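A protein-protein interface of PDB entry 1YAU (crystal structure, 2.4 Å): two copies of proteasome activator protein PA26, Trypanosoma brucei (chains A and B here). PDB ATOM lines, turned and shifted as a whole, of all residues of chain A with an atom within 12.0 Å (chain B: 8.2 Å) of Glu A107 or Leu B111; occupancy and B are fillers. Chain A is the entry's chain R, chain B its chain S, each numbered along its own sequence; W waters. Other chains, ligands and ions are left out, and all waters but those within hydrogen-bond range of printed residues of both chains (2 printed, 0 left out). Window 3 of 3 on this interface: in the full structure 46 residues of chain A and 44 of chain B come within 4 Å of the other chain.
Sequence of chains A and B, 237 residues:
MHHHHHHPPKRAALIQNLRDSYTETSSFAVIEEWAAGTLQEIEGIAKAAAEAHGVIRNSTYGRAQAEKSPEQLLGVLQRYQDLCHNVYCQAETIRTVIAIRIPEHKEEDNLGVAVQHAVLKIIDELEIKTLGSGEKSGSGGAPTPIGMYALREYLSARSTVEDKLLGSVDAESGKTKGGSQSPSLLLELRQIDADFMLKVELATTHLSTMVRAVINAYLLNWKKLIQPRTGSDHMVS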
ATOM      1  N   ILE A 102     -12.108   6.409  23.499  1.00  0.00           N
ATOM      2  CA  ILE A 102     -12.803   6.853  22.307  1.00  0.00           C
ATOM      3  C   ILE A 102     -12.249   8.226  22.144  1.00  0.00           C
ATOM      4  O   ILE A 102     -12.251   8.962  23.110  1.00  0.00           O
ATOM      5  CB  ILE A 102     -14.340   6.844  22.519  1.00  0.00           C
ATOM      6  CG1 ILE A 102     -14.879   5.419  22.373  1.00  0.00           C
ATOM      7  CG2 ILE A 102     -15.082   7.715  21.469  1.00  0.00           C
ATOM      8  CD1 ILE A 102     -16.120   5.191  23.129  1.00  0.00           C
ATOM      9  N   PRO A 103     -11.685   8.563  20.973  1.00  0.00           N
ATOM     10  CA  PRO A 103     -10.947   9.806  20.828  1.00  0.00           C
ATOM     11  C   PRO A 103     -11.885  10.983  20.511  1.00  0.00           C
ATOM     12  O   PRO A 103     -13.099  10.799  20.364  1.00  0.00           O
ATOM     13  CB  PRO A 103     -10.041   9.511  19.643  1.00  0.00           C
ATOM     14  CG  PRO A 103     -10.844   8.660  18.784  1.00  0.00           C
ATOM     15  CD  PRO A 103     -11.698   7.819  19.704  1.00  0.00           C
ATOM     16  N   GLU A 104     -11.310  12.175  20.426  1.00  0.00           N
ATOM     17  CA  GLU A 104     -12.046  13.389  20.051  1.00  0.00           C
ATOM     18  C   GLU A 104     -12.953  13.151  18.841  1.00  0.00           C
ATOM     19  O   GLU A 104     -12.513  12.573  17.840  1.00  0.00           O
ATOM     20  CB  GLU A 104     -11.037  14.478  19.763  1.00  0.00           C
ATOM     21  CG  GLU A 104     -11.596  15.775  19.265  1.00  0.00           C
ATOM     22  CD  GLU A 104     -10.482  16.649  18.765  1.00  0.00           C
ATOM     23  OE1 GLU A 104      -9.331  16.291  19.009  1.00  0.00           O
ATOM     24  OE2 GLU A 104     -10.724  17.649  18.084  1.00  0.00           O
ATOM     25  N   HIS A 105     -14.221  13.570  18.954  1.00  0.00           N
ATOM     26  CA  HIS A 105     -15.212  13.352  17.895  1.00  0.00           C
ATOM     27  C   HIS A 105     -14.875  14.014  16.536  1.00  0.00           C
ATOM     28  O   HIS A 105     -14.733  15.224  16.425  1.00  0.00           O
ATOM     29  CB  HIS A 105     -16.621  13.764  18.352  1.00  0.00           C
ATOM     30  CG  HIS A 105     -17.661  13.570  17.292  1.00  0.00           C
ATOM     31  ND1 HIS A 105     -18.525  12.494  17.288  1.00  0.00           N
ATOM     32  CD2 HIS A 105     -17.929  14.283  16.162  1.00  0.00           C
ATOM     33  CE1 HIS A 105     -19.290  12.560  16.208  1.00  0.00           C
ATOM     34  NE2 HIS A 105     -18.943  13.635  15.508  1.00  0.00           N
ATOM     35  N   LYS A 106     -14.744  13.212  15.495  1.00  0.00           N
ATOM     36  CA  LYS A 106     -14.339  13.778  14.230  1.00  0.00           C
ATOM     37  C   LYS A 106     -15.130  13.153  13.082  1.00  0.00           C
ATOM     38  O   LYS A 106     -15.648  12.046  13.193  1.00  0.00           O
ATOM     39  CB  LYS A 106     -12.827  13.585  14.006  1.00  0.00           C
ATOM     40  CG  LYS A 106     -11.949  14.655  14.600  1.00  0.00           C
ATOM     41  CD  LYS A 106     -10.492  14.371  14.266  1.00  0.00           C
ATOM     42  CE  LYS A 106      -9.540  15.115  15.166  1.00  0.00           C
ATOM     43  NZ  LYS A 106      -9.637  16.624  14.971  1.00  0.00           N
ATOM     44  N   GLU A 107     -15.198  13.859  11.963  1.00  0.00           N
ATOM     45  CA  GLU A 107     -15.852  13.307  10.791  1.00  0.00           C
ATOM     46  C   GLU A 107     -14.793  12.648   9.889  1.00  0.00           C
ATOM     47  O   GLU A 107     -15.049  12.383   8.727  1.00  0.00           O
ATOM     48  CB  GLU A 107     -16.673  14.386  10.038  1.00  0.00           C
ATOM     49  CG  GLU A 107     -17.617  15.246  10.893  1.00  0.00           C
ATOM     50  CD  GLU A 107     -18.730  14.450  11.581  1.00  0.00           C
ATOM     51  OE1 GLU A 107     -19.288  13.523  10.955  1.00  0.00           O
ATOM     52  OE2 GLU A 107     -19.058  14.742  12.746  1.00  0.00           O
ATOM     53  N   GLU A 108     -13.611  12.378  10.421  1.00  0.00           N
ATOM     54  CA  GLU A 108     -12.535  11.750   9.632  1.00  0.00           C
ATOM     55  C   GLU A 108     -11.650  10.942  10.560  1.00  0.00           C
ATOM     56  O   GLU A 108     -11.728  11.137  11.773  1.00  0.00           O
ATOM     57  CB  GLU A 108     -11.699  12.818   8.887  1.00  0.00           C
ATOM     58  CG  GLU A 108     -10.737  13.620   9.764  1.00  0.00           C
ATOM     59  CD  GLU A 108     -10.256  14.883   9.084  1.00  0.00           C
ATOM     60  OE1 GLU A 108      -9.031  15.052   8.878  1.00  0.00           O
ATOM     61  OE2 GLU A 108     -11.124  15.719   8.734  1.00  0.00           O
ATOM     62  N   ASP A 109     -10.808  10.051  10.006  1.00  0.00           N
ATOM     63  CA  ASP A 109      -9.837   9.294  10.798  1.00  0.00           C
ATOM     64  C   ASP A 109     -10.567   8.471  11.873  1.00  0.00           C
ATOM     65  O   ASP A 109     -10.218   8.508  13.062  1.00  0.00           O
ATOM     66  CB  ASP A 109      -8.830  10.256  11.436  1.00  0.00           C
ATOM     67  CG  ASP A 109      -7.556   9.562  11.905  1.00  0.00           C
ATOM     68  OD1 ASP A 109      -7.351   8.357  11.621  1.00  0.00           O
ATOM     69  OD2 ASP A 109      -6.671  10.157  12.552  1.00  0.00           O
ATOM     70  N   ASN A 110     -11.598   7.757  11.429  1.00  0.00           N
ATOM     71  CA  ASN A 110     -12.416   6.928  12.280  1.00  0.00           C
ATOM     72  C   ASN A 110     -12.349   5.417  12.053  1.00  0.00           C
ATOM     73  O   ASN A 110     -13.219   4.695  12.556  1.00  0.00           O
ATOM     74  CB  ASN A 110     -13.882   7.388  12.208  1.00  0.00           C
ATOM     75  CG  ASN A 110     -14.113   8.742  12.896  1.00  0.00           C
ATOM     76  OD1 ASN A 110     -13.505   9.054  13.948  1.00  0.00           O
ATOM     77  ND2 ASN A 110     -14.987   9.555  12.300  1.00  0.00           N
ATOM     78  N   LEU A 111     -11.342   4.923  11.341  1.00  0.00           N
ATOM     79  CA  LEU A 111     -11.191   3.462  11.183  1.00  0.00           C
ATOM     80  C   LEU A 111     -10.994   2.709  12.526  1.00  0.00           C
ATOM     81  O   LEU A 111     -11.618   1.673  12.747  1.00  0.00           O
ATOM     82  CB  LEU A 111     -10.041   3.099  10.215  1.00  0.00           C
ATOM     83  CG  LEU A 111     -10.056   3.763   8.812  1.00  0.00           C
ATOM     84  CD1 LEU A 111      -8.724   3.545   8.094  1.00  0.00           C
ATOM     85  CD2 LEU A 111     -11.260   3.333   7.968  1.00  0.00           C
ATOM     86  N   GLY A 112     -10.132   3.242  13.392  1.00  0.00           N
ATOM     87  CA  GLY A 112      -9.940   2.718  14.725  1.00  0.00           C
ATOM     88  C   GLY A 112     -11.193   2.876  15.572  1.00  0.00           C
ATOM     89  O   GLY A 112     -11.622   1.933  16.265  1.00  0.00           O
ATOM     90  N   VAL A 113     -11.793   4.062  15.523  1.00  0.00           N
ATOM     91  CA  VAL A 113     -13.027   4.328  16.262  1.00  0.00           C
ATOM     92  C   VAL A 113     -14.091   3.309  15.861  1.00  0.00           C
ATOM     93  O   VAL A 113     -14.879   2.870  16.700  1.00  0.00           O
ATOM     94  CB  VAL A 113     -13.496   5.769  16.043  1.00  0.00           C
ATOM     95  CG1 VAL A 113     -14.904   6.004  16.625  1.00  0.00           C
ATOM     96  CG2 VAL A 113     -12.486   6.726  16.628  1.00  0.00           C
ATOM     97  N   ALA A 114     -14.104   2.903  14.591  1.00  0.00           N
ATOM     98  CA  ALA A 114     -15.066   1.906  14.151  1.00  0.00           C
ATOM     99  C   ALA A 114     -14.790   0.518  14.806  1.00  0.00           C
ATOM    100  O   ALA A 114     -15.715  -0.213  15.122  1.00  0.00           O
ATOM    101  CB  ALA A 114     -15.083   1.803  12.615  1.00  0.00           C
ATOM    102  N   HIS A 117     -16.169   0.668  18.467  1.00  0.00           N
ATOM    103  CA  HIS A 117     -17.622   0.535  18.510  1.00  0.00           C
ATOM    104  C   HIS A 117     -18.034  -0.886  18.163  1.00  0.00           C
ATOM    105  O   HIS A 117     -18.959  -1.423  18.767  1.00  0.00           O
ATOM    106  CB  HIS A 117     -18.390   1.592  17.634  1.00  0.00           C
ATOM    107  CG  HIS A 117     -18.237   3.013  18.110  1.00  0.00           C
ATOM    108  ND1 HIS A 117     -18.460   3.397  19.421  1.00  0.00           N
ATOM    109  CD2 HIS A 117     -17.872   4.148  17.449  1.00  0.00           C
ATOM    110  CE1 HIS A 117     -18.217   4.696  19.550  1.00  0.00           C
ATOM    111  NE2 HIS A 117     -17.860   5.176  18.370  1.00  0.00           N
ATOM    112  N   ARG A 229      -6.129   6.096  16.804  1.00  0.00           N
ATOM    113  CA  ARG A 229      -5.484   6.985  15.805  1.00  0.00           C
ATOM    114  C   ARG A 229      -3.954   6.966  15.928  1.00  0.00           C
ATOM    115  O   ARG A 229      -3.429   6.810  17.017  1.00  0.00           O
ATOM    116  CB  ARG A 229      -5.987   8.444  15.934  1.00  0.00           C
ATOM    117  CG  ARG A 229      -7.451   8.603  15.715  1.00  0.00           C
ATOM    118  CD  ARG A 229      -7.967  10.020  15.765  1.00  0.00           C
ATOM    119  NE  ARG A 229      -9.373   9.993  15.369  1.00  0.00           N
ATOM    120  CZ  ARG A 229     -10.356  10.719  15.883  1.00  0.00           C
ATOM    121  NH1 ARG A 229     -10.116  11.601  16.833  1.00  0.00           N
ATOM    122  NH2 ARG A 229     -11.597  10.531  15.455  1.00  0.00           N
ATOM    123  N   GLU B 108     -24.665  23.503   6.906  1.00  0.00           N
ATOM    124  CA  GLU B 108     -23.210  23.497   6.717  1.00  0.00           C
ATOM    125  C   GLU B 108     -22.525  23.903   8.011  1.00  0.00           C
ATOM    126  O   GLU B 108     -23.222  24.323   8.954  1.00  0.00           O
ATOM    127  CB  GLU B 108     -22.803  24.488   5.618  1.00  0.00           C
ATOM    128  CG  GLU B 108     -22.988  25.967   5.983  1.00  0.00           C
ATOM    129  CD  GLU B 108     -22.807  26.879   4.763  1.00  0.00           C
ATOM    130  OE1 GLU B 108     -21.839  27.695   4.720  1.00  0.00           O
ATOM    131  OE2 GLU B 108     -23.625  26.734   3.819  1.00  0.00           O
ATOM    132  N   ASP B 109     -21.186  23.828   8.046  1.00  0.00           N
ATOM    133  CA  ASP B 109     -20.405  24.244   9.219  1.00  0.00           C
ATOM    134  C   ASP B 109     -20.998  23.614  10.511  1.00  0.00           C
ATOM    135  O   ASP B 109     -21.241  24.306  11.512  1.00  0.00           O
ATOM    136  CB  ASP B 109     -20.410  25.771   9.315  1.00  0.00           C
ATOM    137  CG  ASP B 109     -19.313  26.309  10.184  1.00  0.00           C
ATOM    138  OD1 ASP B 109     -18.433  25.527  10.598  1.00  0.00           O
ATOM    139  OD2 ASP B 109     -19.227  27.512  10.515  1.00  0.00           O
ATOM    140  N   ASN B 110     -21.264  22.309  10.441  1.00  0.00           N
ATOM    141  CA  ASN B 110     -21.818  21.528  11.526  1.00  0.00           C
ATOM    142  C   ASN B 110     -20.869  20.472  12.119  1.00  0.00           C
ATOM    143  O   ASN B 110     -21.345  19.493  12.723  1.00  0.00           O
ATOM    144  CB  ASN B 110     -23.104  20.810  11.043  1.00  0.00           C
ATOM    145  CG  ASN B 110     -24.285  21.772  10.864  1.00  0.00           C
ATOM    146  OD1 ASN B 110     -24.486  22.710  11.648  1.00  0.00           O
ATOM    147  ND2 ASN B 110     -25.050  21.551   9.818  1.00  0.00           N
ATOM    148  N   LEU B 111     -19.553  20.632  11.972  1.00  0.00           N
ATOM    149  CA  LEU B 111     -18.653  19.619  12.569  1.00  0.00           C
ATOM    150  C   LEU B 111     -18.725  19.706  14.117  1.00  0.00           C
ATOM    151  O   LEU B 111     -18.953  18.695  14.778  1.00  0.00           O
ATOM    152  CB  LEU B 111     -17.208  19.689  12.016  1.00  0.00           C
ATOM    153  CG  LEU B 111     -17.002  19.682  10.464  1.00  0.00           C
ATOM    154  CD1 LEU B 111     -15.623  20.258  10.067  1.00  0.00           C
ATOM    155  CD2 LEU B 111     -17.183  18.333   9.816  1.00  0.00           C
ATOM    156  N   GLY B 112     -18.620  20.910  14.676  1.00  0.00           N
ATOM    157  CA  GLY B 112     -18.792  21.099  16.101  1.00  0.00           C
ATOM    158  C   GLY B 112     -20.192  20.812  16.622  1.00  0.00           C
ATOM    159  O   GLY B 112     -20.346  20.308  17.736  1.00  0.00           O
ATOM    160  N   VAL B 113     -21.228  21.186  15.869  1.00  0.00           N
ATOM    161  CA  VAL B 113     -22.606  20.850  16.223  1.00  0.00           C
ATOM    162  C   VAL B 113     -22.766  19.334  16.386  1.00  0.00           C
ATOM    163  O   VAL B 113     -23.519  18.860  17.245  1.00  0.00           O
ATOM    164  CB  VAL B 113     -23.599  21.394  15.123  1.00  0.00           C
ATOM    165  CG1 VAL B 113     -24.971  20.826  15.270  1.00  0.00           C
ATOM    166  CG2 VAL B 113     -23.623  22.885  15.121  1.00  0.00           C
ATOM    167  N   ALA B 114     -22.085  18.576  15.525  1.00  0.00           N
ATOM    168  CA  ALA B 114     -22.124  17.093  15.577  1.00  0.00           C
ATOM    169  C   ALA B 114     -21.506  16.579  16.858  1.00  0.00           C
ATOM    170  O   ALA B 114     -21.983  15.608  17.403  1.00  0.00           O
ATOM    171  CB  ALA B 114     -21.440  16.425  14.334  1.00  0.00           C
ATOM    172  N   VAL B 115     -20.446  17.231  17.317  1.00  0.00           N
ATOM    173  CA  VAL B 115     -19.829  16.910  18.615  1.00  0.00           C
ATOM    174  C   VAL B 115     -20.880  17.163  19.724  1.00  0.00           C
ATOM    175  O   VAL B 115     -21.077  16.336  20.630  1.00  0.00           O
ATOM    176  CB  VAL B 115     -18.567  17.802  18.860  1.00  0.00           C
ATOM    177  CG1 VAL B 115     -17.871  17.462  20.189  1.00  0.00           C
ATOM    178  CG2 VAL B 115     -17.602  17.719  17.654  1.00  0.00           C
ATOM    179  N   GLN B 116     -21.575  18.298  19.630  1.00  0.00           N
ATOM    180  CA  GLN B 116     -22.512  18.699  20.672  1.00  0.00           C
ATOM    181  C   GLN B 116     -23.575  17.650  20.787  1.00  0.00           C
ATOM    182  O   GLN B 116     -23.859  17.179  21.882  1.00  0.00           O
ATOM    183  CB  GLN B 116     -23.118  20.059  20.373  1.00  0.00           C
ATOM    184  CG  GLN B 116     -22.198  21.214  20.662  1.00  0.00           C
ATOM    185  CD  GLN B 116     -22.822  22.551  20.303  1.00  0.00           C
ATOM    186  OE1 GLN B 116     -23.429  22.695  19.246  1.00  0.00           O
ATOM    187  NE2 GLN B 116     -22.642  23.536  21.162  1.00  0.00           N
ATOM    188  N   HIS B 117     -24.156  17.277  19.646  1.00  0.00           N
ATOM    189  CA  HIS B 117     -25.173  16.223  19.621  1.00  0.00           C
ATOM    190  C   HIS B 117     -24.664  14.858  20.125  1.00  0.00           C
ATOM    191  O   HIS B 117     -25.354  14.227  20.906  1.00  0.00           O
ATOM    192  CB  HIS B 117     -25.859  16.134  18.237  1.00  0.00           C
ATOM    193  CG  HIS B 117     -26.693  17.351  17.905  1.00  0.00           C
ATOM    194  ND1 HIS B 117     -27.548  17.950  18.814  1.00  0.00           N
ATOM    195  CD2 HIS B 117     -26.783  18.096  16.772  1.00  0.00           C
ATOM    196  CE1 HIS B 117     -28.132  18.999  18.256  1.00  0.00           C
ATOM    197  NE2 HIS B 117     -27.682  19.112  17.019  1.00  0.00           N
ATOM    198  N   ALA B 118     -23.491  14.410  19.654  1.00  0.00           N
ATOM    199  CA  ALA B 118     -22.807  13.179  20.131  1.00  0.00           C
ATOM    200  C   ALA B 118     -22.606  13.120  21.645  1.00  0.00           C
ATOM    201  O   ALA B 118     -22.856  12.097  22.253  1.00  0.00           O
ATOM    202  CB  ALA B 118     -21.432  13.022  19.447  1.00  0.00           C
ATOM    203  N   ASN B 221     -13.645  16.897  24.171  1.00  0.00           N
ATOM    204  CA  ASN B 221     -14.449  17.591  23.175  1.00  0.00           C
ATOM    205  C   ASN B 221     -14.911  18.988  23.599  1.00  0.00           C
ATOM    206  O   ASN B 221     -15.604  19.667  22.838  1.00  0.00           O
ATOM    207  CB  ASN B 221     -15.654  16.746  22.803  1.00  0.00           C
ATOM    208  CG  ASN B 221     -15.296  15.548  21.985  1.00  0.00           C
ATOM    209  OD1 ASN B 221     -14.905  15.658  20.798  1.00  0.00           O
ATOM    210  ND2 ASN B 221     -15.505  14.378  22.565  1.00  0.00           N
ATOM    211  N   LYS B 224     -15.233  22.516  21.362  1.00  0.00           N
ATOM    212  CA  LYS B 224     -16.311  22.467  20.368  1.00  0.00           C
ATOM    213  C   LYS B 224     -17.713  22.413  20.970  1.00  0.00           C
ATOM    214  O   LYS B 224     -18.681  22.832  20.331  1.00  0.00           O
ATOM    215  CB  LYS B 224     -16.102  21.282  19.437  1.00  0.00           C
ATOM    216  CG  LYS B 224     -14.850  21.435  18.534  1.00  0.00           C
ATOM    217  CD  LYS B 224     -15.274  21.882  17.176  1.00  0.00           C
ATOM    218  CE  LYS B 224     -14.097  21.953  16.208  1.00  0.00           C
ATOM    219  NZ  LYS B 224     -13.713  23.383  15.960  1.00  0.00           N
ATOM    220  N   LEU B 225     -17.818  21.886  22.194  1.00  0.00           N
ATOM    221  CA  LEU B 225     -19.033  21.994  22.983  1.00  0.00           C
ATOM    222  C   LEU B 225     -19.420  23.446  23.316  1.00  0.00           C
ATOM    223  O   LEU B 225     -20.584  23.759  23.348  1.00  0.00           O
ATOM    224  CB  LEU B 225     -18.952  21.139  24.263  1.00  0.00           C
ATOM    225  CG  LEU B 225     -18.759  19.615  24.104  1.00  0.00           C
ATOM    226  CD1 LEU B 225     -18.673  18.864  25.485  1.00  0.00           C
ATOM    227  CD2 LEU B 225     -19.855  19.015  23.232  1.00  0.00           C
ATOM    228  N   GLN B 227     -17.689  26.467  21.828  1.00  0.00           N
ATOM    229  CA  GLN B 227     -17.628  27.198  20.573  1.00  0.00           C
ATOM    230  C   GLN B 227     -17.612  26.222  19.372  1.00  0.00           C
ATOM    231  O   GLN B 227     -16.561  25.918  18.845  1.00  0.00           O
ATOM    232  CB  GLN B 227     -16.409  28.146  20.524  1.00  0.00           C
ATOM    233  CG  GLN B 227     -16.232  29.052  21.788  1.00  0.00           C
ATOM    234  CD  GLN B 227     -17.285  30.201  21.908  1.00  0.00           C
ATOM    235  OE1 GLN B 227     -17.916  30.605  20.893  1.00  0.00           O
ATOM    236  NE2 GLN B 227     -17.471  30.723  23.149  1.00  0.00           N
ATOM    237  N   PRO B 228     -18.787  25.768  18.913  1.00  0.00           N
ATOM    238  CA  PRO B 228     -18.870  24.774  17.812  1.00  0.00           C
ATOM    239  C   PRO B 228     -18.472  25.303  16.435  1.00  0.00           C
ATOM    240  O   PRO B 228     -18.252  24.500  15.524  1.00  0.00           O
ATOM    241  CB  PRO B 228     -20.353  24.386  17.778  1.00  0.00           C
ATOM    242  CG  PRO B 228     -21.082  25.342  18.653  1.00  0.00           C
ATOM    243  CD  PRO B 228     -20.116  26.196  19.406  1.00  0.00           C
ATOM    244  N   ARG B 229     -18.425  26.635  16.277  1.00  0.00           N
ATOM    245  CA  ARG B 229     -18.066  27.282  15.014  1.00  0.00           C
ATOM    246  C   ARG B 229     -17.028  28.354  15.276  1.00  0.00           C
ATOM    247  O   ARG B 229     -17.132  29.081  16.258  1.00  0.00           O
ATOM    248  CB  ARG B 229     -19.301  27.889  14.328  1.00  0.00           C
ATOM    249  CG  ARG B 229     -20.332  26.861  13.858  1.00  0.00           C
ATOM    250  CD  ARG B 229     -21.533  27.484  13.163  1.00  0.00           C
ATOM    251  NE  ARG B 229     -22.462  26.471  12.658  1.00  0.00           N
ATOM    252  CZ  ARG B 229     -23.772  26.609  12.560  1.00  0.00           C
ATOM    253  NH1 ARG B 229     -24.404  27.730  12.958  1.00  0.00           N
ATOM    254  NH2 ARG B 229     -24.475  25.597  12.097  1.00  0.00           N
HETATM  255  O   HOH W   1     -17.162  16.159  14.034  1.00  0.00           O
HETATM  256  O   HOH W   2     -15.374  11.668  21.579  1.00  0.00           O
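The backbone NH of His A105 lies within hydrogen-bond range of the side-chain amide oxygen of Asn B221 (2.9 Å).
The side-chain carboxylate (OE2) of Glu A104 lies within salt-bridge range of the side-chain amino group (NZ) of Lys A106 (3.5 Å). O of Glu A104 is in hydrogen-bond range of NH1 of Arg A229, 2.8 Å away. A ring nitrogen (NE2) of His A105 is in hydrogen-bond range of the side-chain carboxylate (OE2) of Glu A107.
Glu A104 touches Asn B221. His A105 touches Ala B114 (NE2 to CB, 3.9 Å). His A105 touches Val B115. His A105 touches Ala B118 (ND1 to CB, 3.7 Å). CG of Glu A107 touches CD2 of Leu B111 (3.3 Å). OE2 of Glu A107 touches CB of Ala B114, 3.3 Å away.
Of the printed residues of chain B, Glu A104 touches Asn B221. Printed residues of chain B within 4 Å of His A105: Ala B114 (3.9 Å), Val B115 (3.8 Å), Ala B118 (3.7 Å) and Asn B221 (2.9 Å). Glu A107 touches just these residues of chain B: Leu B111 and Ala B114. No residue of chain A comes within 4 Å of Asp B109. Of chain A, only Glu A107 (3.3 Å) comes within 4 Å of Leu B111. No residue of chain A comes within 4 Å of Val B113. Ala B114 touches two residues of chain A. Of the printed residues of chain A, Ala B118 touches His A105. Of the printed residues of chain A, Asn B221 touches Glu A104 (3.6 Å) and His A105 (2.9 Å). The nearest residue of chain B that does not touch Glu A107 is Asn B110 (5.3 Å). The nearest residue of chain A that does not touch Leu B111 is His A105 (4.7 Å).
Hydrophobic or aromatic side chains of chain A within 4 Å of the printed part of chain B: His A105. Among the printed residues, 7 pairs touch across the chains.
9 positions are printed for both chains. Of the 7 pairs that touch across the chains among the printed residues, none has its exchanged pair printed and touching as well.
Water W1 lies within hydrogen-bond range of OE2 of Glu A107 (2.7 Å), O of Leu B111 (3.2 Å) and NE2 of His A105 (3.4 Å). Water W2 lies within hydrogen-bond range of the backbone carbonyl oxygen of Pro A103, the side-chain amide nitrogen of Asn B221 and the backbone NH of His A105.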
